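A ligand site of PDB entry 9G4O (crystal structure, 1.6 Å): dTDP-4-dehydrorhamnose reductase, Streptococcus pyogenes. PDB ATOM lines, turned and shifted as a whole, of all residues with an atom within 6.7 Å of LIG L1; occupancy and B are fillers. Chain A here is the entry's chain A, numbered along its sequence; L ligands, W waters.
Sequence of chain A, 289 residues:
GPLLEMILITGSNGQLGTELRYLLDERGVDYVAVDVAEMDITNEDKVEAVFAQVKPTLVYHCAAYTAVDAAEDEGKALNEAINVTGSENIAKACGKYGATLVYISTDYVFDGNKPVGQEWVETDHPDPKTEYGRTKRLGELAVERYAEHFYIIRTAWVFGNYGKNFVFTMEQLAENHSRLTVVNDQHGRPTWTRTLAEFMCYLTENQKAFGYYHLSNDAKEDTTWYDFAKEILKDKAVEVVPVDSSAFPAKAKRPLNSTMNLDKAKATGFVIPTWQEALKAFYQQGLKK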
ATOM      1  N   THR A  66       5.806   1.844  27.749  1.00  0.00           N
ATOM      2  CA  THR A  66       5.647   0.469  28.228  1.00  0.00           C
ATOM      3  C   THR A  66       5.921   0.321  29.719  1.00  0.00           C
ATOM      4  O   THR A  66       6.132  -0.808  30.189  1.00  0.00           O
ATOM      5  CB  THR A  66       6.544  -0.478  27.418  1.00  0.00           C
ATOM      6  OG1 THR A  66       7.917  -0.165  27.686  1.00  0.00           O
ATOM      7  CG2 THR A  66       6.285  -0.311  25.949  1.00  0.00           C
ATOM      8  N   ALA A  67       5.886   1.409  30.486  1.00  0.00           N
ATOM      9  CA  ALA A  67       6.012   1.349  31.946  1.00  0.00           C
ATOM     10  C   ALA A  67       4.639   1.046  32.520  1.00  0.00           C
ATOM     11  O   ALA A  67       3.811   1.946  32.665  1.00  0.00           O
ATOM     12  CB  ALA A  67       6.584   2.646  32.501  1.00  0.00           C
ATOM     13  N   VAL A  68       4.371  -0.221  32.817  1.00  0.00           N
ATOM     14  CA  VAL A  68       3.002  -0.634  33.101  1.00  0.00           C
ATOM     15  C   VAL A  68       2.498  -0.003  34.391  1.00  0.00           C
ATOM     16  O   VAL A  68       1.389   0.525  34.454  1.00  0.00           O
ATOM     17  CB  VAL A  68       2.906  -2.166  33.132  1.00  0.00           C
ATOM     18  CG1 VAL A  68       1.546  -2.621  33.650  1.00  0.00           C
ATOM     19  CG2 VAL A  68       3.145  -2.709  31.752  1.00  0.00           C
ATOM     20  N   ASP A  69       3.317  -0.030  35.438  1.00  0.00           N
ATOM     21  CA  ASP A  69       2.855   0.473  36.727  1.00  0.00           C
ATOM     22  C   ASP A  69       2.776   1.994  36.708  1.00  0.00           C
ATOM     23  O   ASP A  69       1.833   2.566  37.238  1.00  0.00           O
ATOM     24  CB  ASP A  69       3.761  -0.040  37.830  1.00  0.00           C
ATOM     25  CG  ASP A  69       3.548  -1.528  38.100  1.00  0.00           C
ATOM     26  OD1 ASP A  69       2.460  -1.913  38.578  1.00  0.00           O
ATOM     27  OD2 ASP A  69       4.447  -2.316  37.741  1.00  0.00           O
ATOM     28  N   ALA A  70       3.732   2.663  36.054  1.00  0.00           N
ATOM     29  CA  ALA A  70       3.685   4.115  35.929  1.00  0.00           C
ATOM     30  C   ALA A  70       2.467   4.586  35.138  1.00  0.00           C
ATOM     31  O   ALA A  70       1.926   5.674  35.404  1.00  0.00           O
ATOM     32  CB  ALA A  70       4.976   4.623  35.281  1.00  0.00           C
ATOM     33  N   THR A 106       0.384  -5.898  22.383  1.00  0.00           N
ATOM     34  CA  THR A 106       0.797  -6.551  23.622  1.00  0.00           C
ATOM     35  C   THR A 106      -0.166  -7.658  24.012  1.00  0.00           C
ATOM     36  O   THR A 106      -1.373  -7.583  23.758  1.00  0.00           O
ATOM     37  CB  THR A 106       0.922  -5.523  24.770  1.00  0.00           C
ATOM     38  OG1 THR A 106       1.264  -6.186  25.976  1.00  0.00           O
ATOM     39  CG2 THR A 106      -0.403  -4.801  25.006  1.00  0.00           C
ATOM     40  N   ASP A 107       0.387  -8.695  24.649  1.00  0.00           N
ATOM     41  CA  ASP A 107      -0.420  -9.691  25.332  1.00  0.00           C
ATOM     42  C   ASP A 107      -1.294  -9.087  26.421  1.00  0.00           C
ATOM     43  O   ASP A 107      -2.304  -9.689  26.805  1.00  0.00           O
ATOM     44  CB  ASP A 107       0.501 -10.797  25.911  1.00  0.00           C
ATOM     45  CG  ASP A 107       1.390 -10.295  27.070  1.00  0.00           C
ATOM     46  OD1 ASP A 107       1.849  -9.129  27.040  1.00  0.00           O
ATOM     47  OD2 ASP A 107       1.647 -11.088  28.001  1.00  0.00           O
ATOM     48  N   TYR A 108      -0.936  -7.885  26.920  1.00  0.00           N
ATOM     49  CA  TYR A 108      -1.760  -7.264  27.936  1.00  0.00           C
ATOM     50  C   TYR A 108      -3.068  -6.692  27.359  1.00  0.00           C
ATOM     51  O   TYR A 108      -3.790  -5.990  28.083  1.00  0.00           O
ATOM     52  CB  TYR A 108      -0.972  -6.174  28.667  1.00  0.00           C
ATOM     53  CG  TYR A 108      -0.066  -6.679  29.807  1.00  0.00           C
ATOM     54  CD1 TYR A 108       0.310  -8.020  29.894  1.00  0.00           C
ATOM     55  CD2 TYR A 108       0.392  -5.803  30.797  1.00  0.00           C
ATOM     56  CE1 TYR A 108       1.134  -8.481  30.943  1.00  0.00           C
ATOM     57  CE2 TYR A 108       1.207  -6.252  31.829  1.00  0.00           C
ATOM     58  CZ  TYR A 108       1.575  -7.588  31.913  1.00  0.00           C
ATOM     59  OH  TYR A 108       2.397  -8.013  32.964  1.00  0.00           O
ATOM     60  N   TYR A 132      -1.995   0.439  30.544  1.00  0.00           N
ATOM     61  CA  TYR A 132      -1.141   0.141  29.406  1.00  0.00           C
ATOM     62  C   TYR A 132      -1.925  -0.652  28.359  1.00  0.00           C
ATOM     63  O   TYR A 132      -2.017  -0.234  27.205  1.00  0.00           O
ATOM     64  CB  TYR A 132       0.103  -0.616  29.900  1.00  0.00           C
ATOM     65  CG  TYR A 132       0.918  -1.227  28.786  1.00  0.00           C
ATOM     66  CD1 TYR A 132       1.612  -0.430  27.885  1.00  0.00           C
ATOM     67  CD2 TYR A 132       0.949  -2.605  28.606  1.00  0.00           C
ATOM     68  CE1 TYR A 132       2.341  -0.979  26.844  1.00  0.00           C
ATOM     69  CE2 TYR A 132       1.672  -3.178  27.570  1.00  0.00           C
ATOM     70  CZ  TYR A 132       2.365  -2.365  26.693  1.00  0.00           C
ATOM     71  OH  TYR A 132       3.084  -2.924  25.656  1.00  0.00           O
ATOM     72  N   THR A 155       2.981  -8.840  21.233  1.00  0.00           N
ATOM     73  CA  THR A 155       4.145  -9.504  21.806  1.00  0.00           C
ATOM     74  C   THR A 155       4.084  -9.402  23.337  1.00  0.00           C
ATOM     75  O   THR A 155       3.129  -8.890  23.911  1.00  0.00           O
ATOM     76  CB  THR A 155       5.441  -8.921  21.229  1.00  0.00           C
ATOM     77  OG1 THR A 155       6.547  -9.764  21.584  1.00  0.00           O
ATOM     78  CG2 THR A 155       5.699  -7.502  21.762  1.00  0.00           C
ATOM     79  N   ALA A 156       5.091  -9.948  24.017  1.00  0.00           N
ATOM     80  CA  ALA A 156       4.997 -10.059  25.469  1.00  0.00           C
ATOM     81  C   ALA A 156       6.353 -10.015  26.119  1.00  0.00           C
ATOM     82  O   ALA A 156       7.293 -10.638  25.628  1.00  0.00           O
ATOM     83  CB  ALA A 156       4.314 -11.361  25.900  1.00  0.00           C
ATOM     84  N   TRP A 157       6.450  -9.350  27.280  1.00  0.00           N
ATOM     85  CA  TRP A 157       7.592  -9.538  28.174  1.00  0.00           C
ATOM     86  C   TRP A 157       8.908  -9.347  27.424  1.00  0.00           C
ATOM     87  O   TRP A 157       9.780 -10.219  27.415  1.00  0.00           O
ATOM     88  CB  TRP A 157       7.554 -10.916  28.829  1.00  0.00           C
ATOM     89  CG  TRP A 157       6.308 -11.293  29.600  1.00  0.00           C
ATOM     90  CD1 TRP A 157       5.059 -10.714  29.539  1.00  0.00           C
ATOM     91  CD2 TRP A 157       6.207 -12.366  30.520  1.00  0.00           C
ATOM     92  NE1 TRP A 157       4.192 -11.371  30.399  1.00  0.00           N
ATOM     93  CE2 TRP A 157       4.889 -12.398  31.006  1.00  0.00           C
ATOM     94  CE3 TRP A 157       7.117 -13.332  30.979  1.00  0.00           C
ATOM     95  CZ2 TRP A 157       4.461 -13.335  31.945  1.00  0.00           C
ATOM     96  CZ3 TRP A 157       6.686 -14.263  31.906  1.00  0.00           C
ATOM     97  CH2 TRP A 157       5.370 -14.259  32.361  1.00  0.00           C
ATOM     98  N   VAL A 158       9.052  -8.191  26.796  1.00  0.00           N
ATOM     99  CA  VAL A 158      10.069  -8.005  25.762  1.00  0.00           C
ATOM    100  C   VAL A 158      11.406  -7.675  26.409  1.00  0.00           C
ATOM    101  O   VAL A 158      11.487  -6.839  27.322  1.00  0.00           O
ATOM    102  CB  VAL A 158       9.648  -6.903  24.779  1.00  0.00           C
ATOM    103  CG1 VAL A 158      10.729  -6.680  23.777  1.00  0.00           C
ATOM    104  CG2 VAL A 158       8.324  -7.282  24.089  1.00  0.00           C
ATOM    105  N   PHE A 166      13.179  -6.294  31.889  1.00  0.00           N
ATOM    106  CA  PHE A 166      13.189  -7.143  33.087  1.00  0.00           C
ATOM    107  C   PHE A 166      14.537  -7.810  33.326  1.00  0.00           C
ATOM    108  O   PHE A 166      14.976  -7.937  34.475  1.00  0.00           O
ATOM    109  CB  PHE A 166      12.110  -8.219  32.968  1.00  0.00           C
ATOM    110  CG  PHE A 166      11.928  -9.047  34.206  1.00  0.00           C
ATOM    111  CD1 PHE A 166      11.380  -8.496  35.368  1.00  0.00           C
ATOM    112  CD2 PHE A 166      12.321 -10.386  34.210  1.00  0.00           C
ATOM    113  CE1 PHE A 166      11.218  -9.264  36.496  1.00  0.00           C
ATOM    114  CE2 PHE A 166      12.157 -11.170  35.347  1.00  0.00           C
ATOM    115  CZ  PHE A 166      11.599 -10.606  36.492  1.00  0.00           C
ATOM    116  N   ARG A 189       4.941 -15.439  28.349  1.00  0.00           N
ATOM    117  CA  ARG A 189       6.227 -15.872  27.840  1.00  0.00           C
ATOM    118  C   ARG A 189       7.102 -14.692  27.440  1.00  0.00           C
ATOM    119  O   ARG A 189       6.617 -13.748  26.799  1.00  0.00           O
ATOM    120  CB  ARG A 189       6.077 -16.792  26.607  1.00  0.00           C
ATOM    121  CG  ARG A 189       5.192 -18.016  26.810  1.00  0.00           C
ATOM    122  CD  ARG A 189       5.070 -18.793  25.516  1.00  0.00           C
ATOM    123  NE  ARG A 189       4.384 -20.067  25.679  1.00  0.00           N
ATOM    124  CZ  ARG A 189       3.346 -20.439  24.938  1.00  0.00           C
ATOM    125  NH1 ARG A 189       2.815 -19.629  24.044  1.00  0.00           N
ATOM    126  NH2 ARG A 189       2.836 -21.650  25.108  1.00  0.00           N
ATOM    127  N   TRP A 225       6.807 -15.167  35.434  1.00  0.00           N
ATOM    128  CA  TRP A 225       7.945 -14.285  35.660  1.00  0.00           C
ATOM    129  C   TRP A 225       9.007 -14.928  36.538  1.00  0.00           C
ATOM    130  O   TRP A 225      10.208 -14.779  36.288  1.00  0.00           O
ATOM    131  CB  TRP A 225       7.495 -12.963  36.287  1.00  0.00           C
ATOM    132  CG  TRP A 225       6.727 -12.065  35.355  1.00  0.00           C
ATOM    133  CD1 TRP A 225       5.379 -11.834  35.360  1.00  0.00           C
ATOM    134  CD2 TRP A 225       7.282 -11.246  34.314  1.00  0.00           C
ATOM    135  NE1 TRP A 225       5.050 -10.929  34.363  1.00  0.00           N
ATOM    136  CE2 TRP A 225       6.205 -10.555  33.714  1.00  0.00           C
ATOM    137  CE3 TRP A 225       8.578 -11.015  33.838  1.00  0.00           C
ATOM    138  CZ2 TRP A 225       6.384  -9.657  32.657  1.00  0.00           C
ATOM    139  CZ3 TRP A 225       8.757 -10.117  32.781  1.00  0.00           C
ATOM    140  CH2 TRP A 225       7.659  -9.452  32.212  1.00  0.00           C
ATOM    141  N   ARG A 254      -2.208  -6.782  36.611  1.00  0.00           N
ATOM    142  CA  ARG A 254      -1.665  -7.466  35.456  1.00  0.00           C
ATOM    143  C   ARG A 254      -2.465  -8.742  35.189  1.00  0.00           C
ATOM    144  O   ARG A 254      -3.014  -9.338  36.117  1.00  0.00           O
ATOM    145  CB  ARG A 254      -0.205  -7.808  35.727  1.00  0.00           C
ATOM    146  CG  ARG A 254       0.669  -6.564  35.778  1.00  0.00           C
ATOM    147  CD  ARG A 254       2.119  -6.895  36.033  1.00  0.00           C
ATOM    148  NE  ARG A 254       2.886  -5.671  36.264  1.00  0.00           N
ATOM    149  CZ  ARG A 254       3.714  -5.132  35.390  1.00  0.00           C
ATOM    150  NH1 ARG A 254       3.947  -5.692  34.204  1.00  0.00           N
ATOM    151  NH2 ARG A 254       4.355  -4.000  35.711  1.00  0.00           N
ATOM    152  N   SER A 258      -1.648 -14.481  30.478  1.00  0.00           N
ATOM    153  CA  SER A 258      -1.668 -13.825  29.182  1.00  0.00           C
ATOM    154  C   SER A 258      -0.813 -14.576  28.182  1.00  0.00           C
ATOM    155  O   SER A 258      -0.259 -13.979  27.246  1.00  0.00           O
ATOM    156  CB  SER A 258      -1.225 -12.359  29.317  1.00  0.00           C
ATOM    157  OG  SER A 258       0.132 -12.301  29.700  1.00  0.00           O
HETATM  158  C1  LIG L   1       5.207  -6.784  30.413  1.00  0.00           C
HETATM  159  C2  LIG L   1       6.159  -6.034  31.099  1.00  0.00           C
HETATM  160  C3  LIG L   1       7.335  -3.829  31.577  1.00  0.00           C
HETATM  161  C4  LIG L   1       6.708  -3.278  32.866  1.00  0.00           C
HETATM  162  C5  LIG L   1       6.294  -4.674  30.827  1.00  0.00           C
HETATM  163  C6  LIG L   1       5.494  -4.059  29.869  1.00  0.00           C
HETATM  164  C7  LIG L   1       4.546  -4.801  29.186  1.00  0.00           C
HETATM  165  C8  LIG L   1       4.411  -6.161  29.458  1.00  0.00           C
HETATM  166  C9  LIG L   1       3.347  -6.939  28.690  1.00  0.00           C
HETATM  167  O1  LIG L   1       5.996  -4.034  33.574  1.00  0.00           O
HETATM  168  O2  LIG L   1       6.873  -2.082  33.214  1.00  0.00           O
HETATM  169  O3  LIG L   1       3.962  -7.922  27.908  1.00  0.00           O
HETATM  170  P1  LG2 L   2      11.078   0.761  24.598  1.00  0.00           P
HETATM  171  O1  LG2 L   2      10.592   1.474  25.814  1.00  0.00           O
HETATM  172  O2  LG2 L   2      12.499   0.154  24.805  1.00  0.00           O
HETATM  173  O3  LG2 L   2      11.321   1.886  23.347  1.00  0.00           O
HETATM  174  C1  LG2 L   2      10.240   2.206  22.493  1.00  0.00           C
HETATM  175  C2  LG2 L   2      10.642   3.589  21.868  1.00  0.00           C
HETATM  176  O4  LG2 L   2       9.392   4.424  21.882  1.00  0.00           O
HETATM  177  C3  LG2 L   2      11.479   4.249  22.651  1.00  0.00           C
HETATM  178  O5  LG2 L   2      12.736   4.509  21.979  1.00  0.00           O
HETATM  179  O6  LG2 L   2      11.605   6.834  23.363  1.00  0.00           O
HETATM  180  C4  LG2 L   2      10.069   5.870  21.978  1.00  0.00           C
HETATM  181  N1  LG2 L   2       9.027   6.910  22.138  1.00  0.00           N
HETATM  182  C5  LG2 L   2       8.253   7.101  23.206  1.00  0.00           C
HETATM  183  N2  LG2 L   2       7.468   8.132  22.957  1.00  0.00           N
HETATM  184  C6  LG2 L   2       7.231   9.646  20.926  1.00  0.00           C
HETATM  185  N3  LG2 L   2       6.154  10.535  21.434  1.00  0.00           N
HETATM  186  N4  LG2 L   2       7.741   9.832  19.706  1.00  0.00           N
HETATM  187  C7  LG2 L   2       8.713   9.028  19.238  1.00  0.00           C
HETATM  188  N5  LG2 L   2       9.220   8.034  19.944  1.00  0.00           N
HETATM  189  C8  LG2 L   2       8.712   7.798  21.194  1.00  0.00           C
HETATM  190  O7  LG2 L   2       9.907  -0.323  24.178  1.00  0.00           O
HETATM  191  P2  LG2 L   2      10.225  -1.759  23.413  1.00  0.00           P
HETATM  192  O8  LG2 L   2      11.409  -1.466  22.491  1.00  0.00           O
HETATM  193  O9  LG2 L   2      10.500  -2.863  24.495  1.00  0.00           O
HETATM  194  O10 LG2 L   2       8.909  -2.309  22.520  1.00  0.00           O
HETATM  195  C9  LG2 L   2       8.229  -1.476  21.610  1.00  0.00           C
HETATM  196  C10 LG2 L   2       6.890  -2.188  21.365  1.00  0.00           C
HETATM  197  O11 LG2 L   2       6.844  -3.561  22.249  1.00  0.00           O
HETATM  198  C11 LG2 L   2       5.925  -1.507  21.777  1.00  0.00           C
HETATM  199  O12 LG2 L   2       4.828  -1.493  20.785  1.00  0.00           O
HETATM  200  C12 LG2 L   2       5.356  -2.254  23.179  1.00  0.00           C
HETATM  201  O13 LG2 L   2       4.031  -1.858  23.451  1.00  0.00           O
HETATM  202  C13 LG2 L   2       5.438  -3.516  22.831  1.00  0.00           C
HETATM  203  N6  LG2 L   2       5.411  -4.389  24.017  1.00  0.00           N
HETATM  204  C14 LG2 L   2       6.446  -4.298  24.890  1.00  0.00           C
HETATM  205  C15 LG2 L   2       6.426  -5.091  26.018  1.00  0.00           C
HETATM  206  C16 LG2 L   2       7.557  -5.095  27.089  1.00  0.00           C
HETATM  207  O14 LG2 L   2       7.630  -6.127  27.755  1.00  0.00           O
HETATM  208  C17 LG2 L   2       5.385  -5.967  26.236  1.00  0.00           C
HETATM  209  C18 LG2 L   2       4.326  -6.036  25.339  1.00  0.00           C
HETATM  210  C19 LG2 L   2       4.395  -5.202  24.198  1.00  0.00           C
HETATM  211  O   HOH W   1       5.976  -1.108  35.489  1.00  0.00           O
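O3 of LIG L1 lies within hydrogen-bond range of OD1 of Asp 107, at 2.6 Å. An oxygen (O1) of LIG L1 is in salt-bridge range of the guanidinium group (NH2) of Arg 254. The backbone NH (N) of Trp 157 sits at hydrogen-bond distance from an oxygen (O3) of LIG L1 (2.9 Å). The backbone NH (N) of Val 68 lies within hydrogen-bond range of an oxygen (O2) of LIG L1 (3.1 Å). An oxygen (O14) of LG2 L2 sits close to the backbone NH (N) of Trp 157 (3.5 Å). An oxygen (O13) of LG2 L2 is in hydrogen-bond range of the side-chain hydroxyl of Tyr 132 (2.6 Å). N of Val 158 is in hydrogen-bond range of O14 of LG2 L2.
OG1 of Thr 106 is in hydrogen-bond range of OD1 of Asp 107 (3.2 Å). N of Asp 107 lies within hydrogen-bond range of O of Thr 155 (2.8 Å). The side-chain carboxylate (OD2) of Asp 107 lies within hydrogen-bond range of the side-chain hydroxyl (OG) of Ser 258 (2.6 Å). OH of Tyr 108 is in hydrogen-bond range of NH1 of Arg 254 (3.1 Å). The guanidinium group (NH2) of Arg 254 lies within salt-bridge range of the side-chain carboxylate (OD2) of Asp 69 (2.6 Å). OG1 of Thr 106 sits at hydrogen-bond distance from N of Tyr 108.
O of Thr 66 sits close to O2 of LIG L1 (3.4 Å). Ala 67 touches LIG L1. OG1 of Thr 106 touches C9 of LIG L1 (3.5 Å). CD1 of Tyr 108 touches C9 of LIG L1, at 3.4 Å. Tyr 132 touches LIG L1 (CE2 to C7, 3.7 Å). Ala 156 touches LIG L1 (CA to O3, 3.4 Å). Trp 225 touches LIG L1 (CZ2 to C1, 3.8 Å). Hydrophobic or aromatic side chains within 4 Å of LIG L1: Val 68, Tyr 108, Tyr 132, Ala 156, Trp 157 and Trp 225. Along chain A the residues within 4 Å of LIG L1 span positions 66 to 254. The nearest printed residue that does not touch LIG L1 is Thr 155 (4.2 Å).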
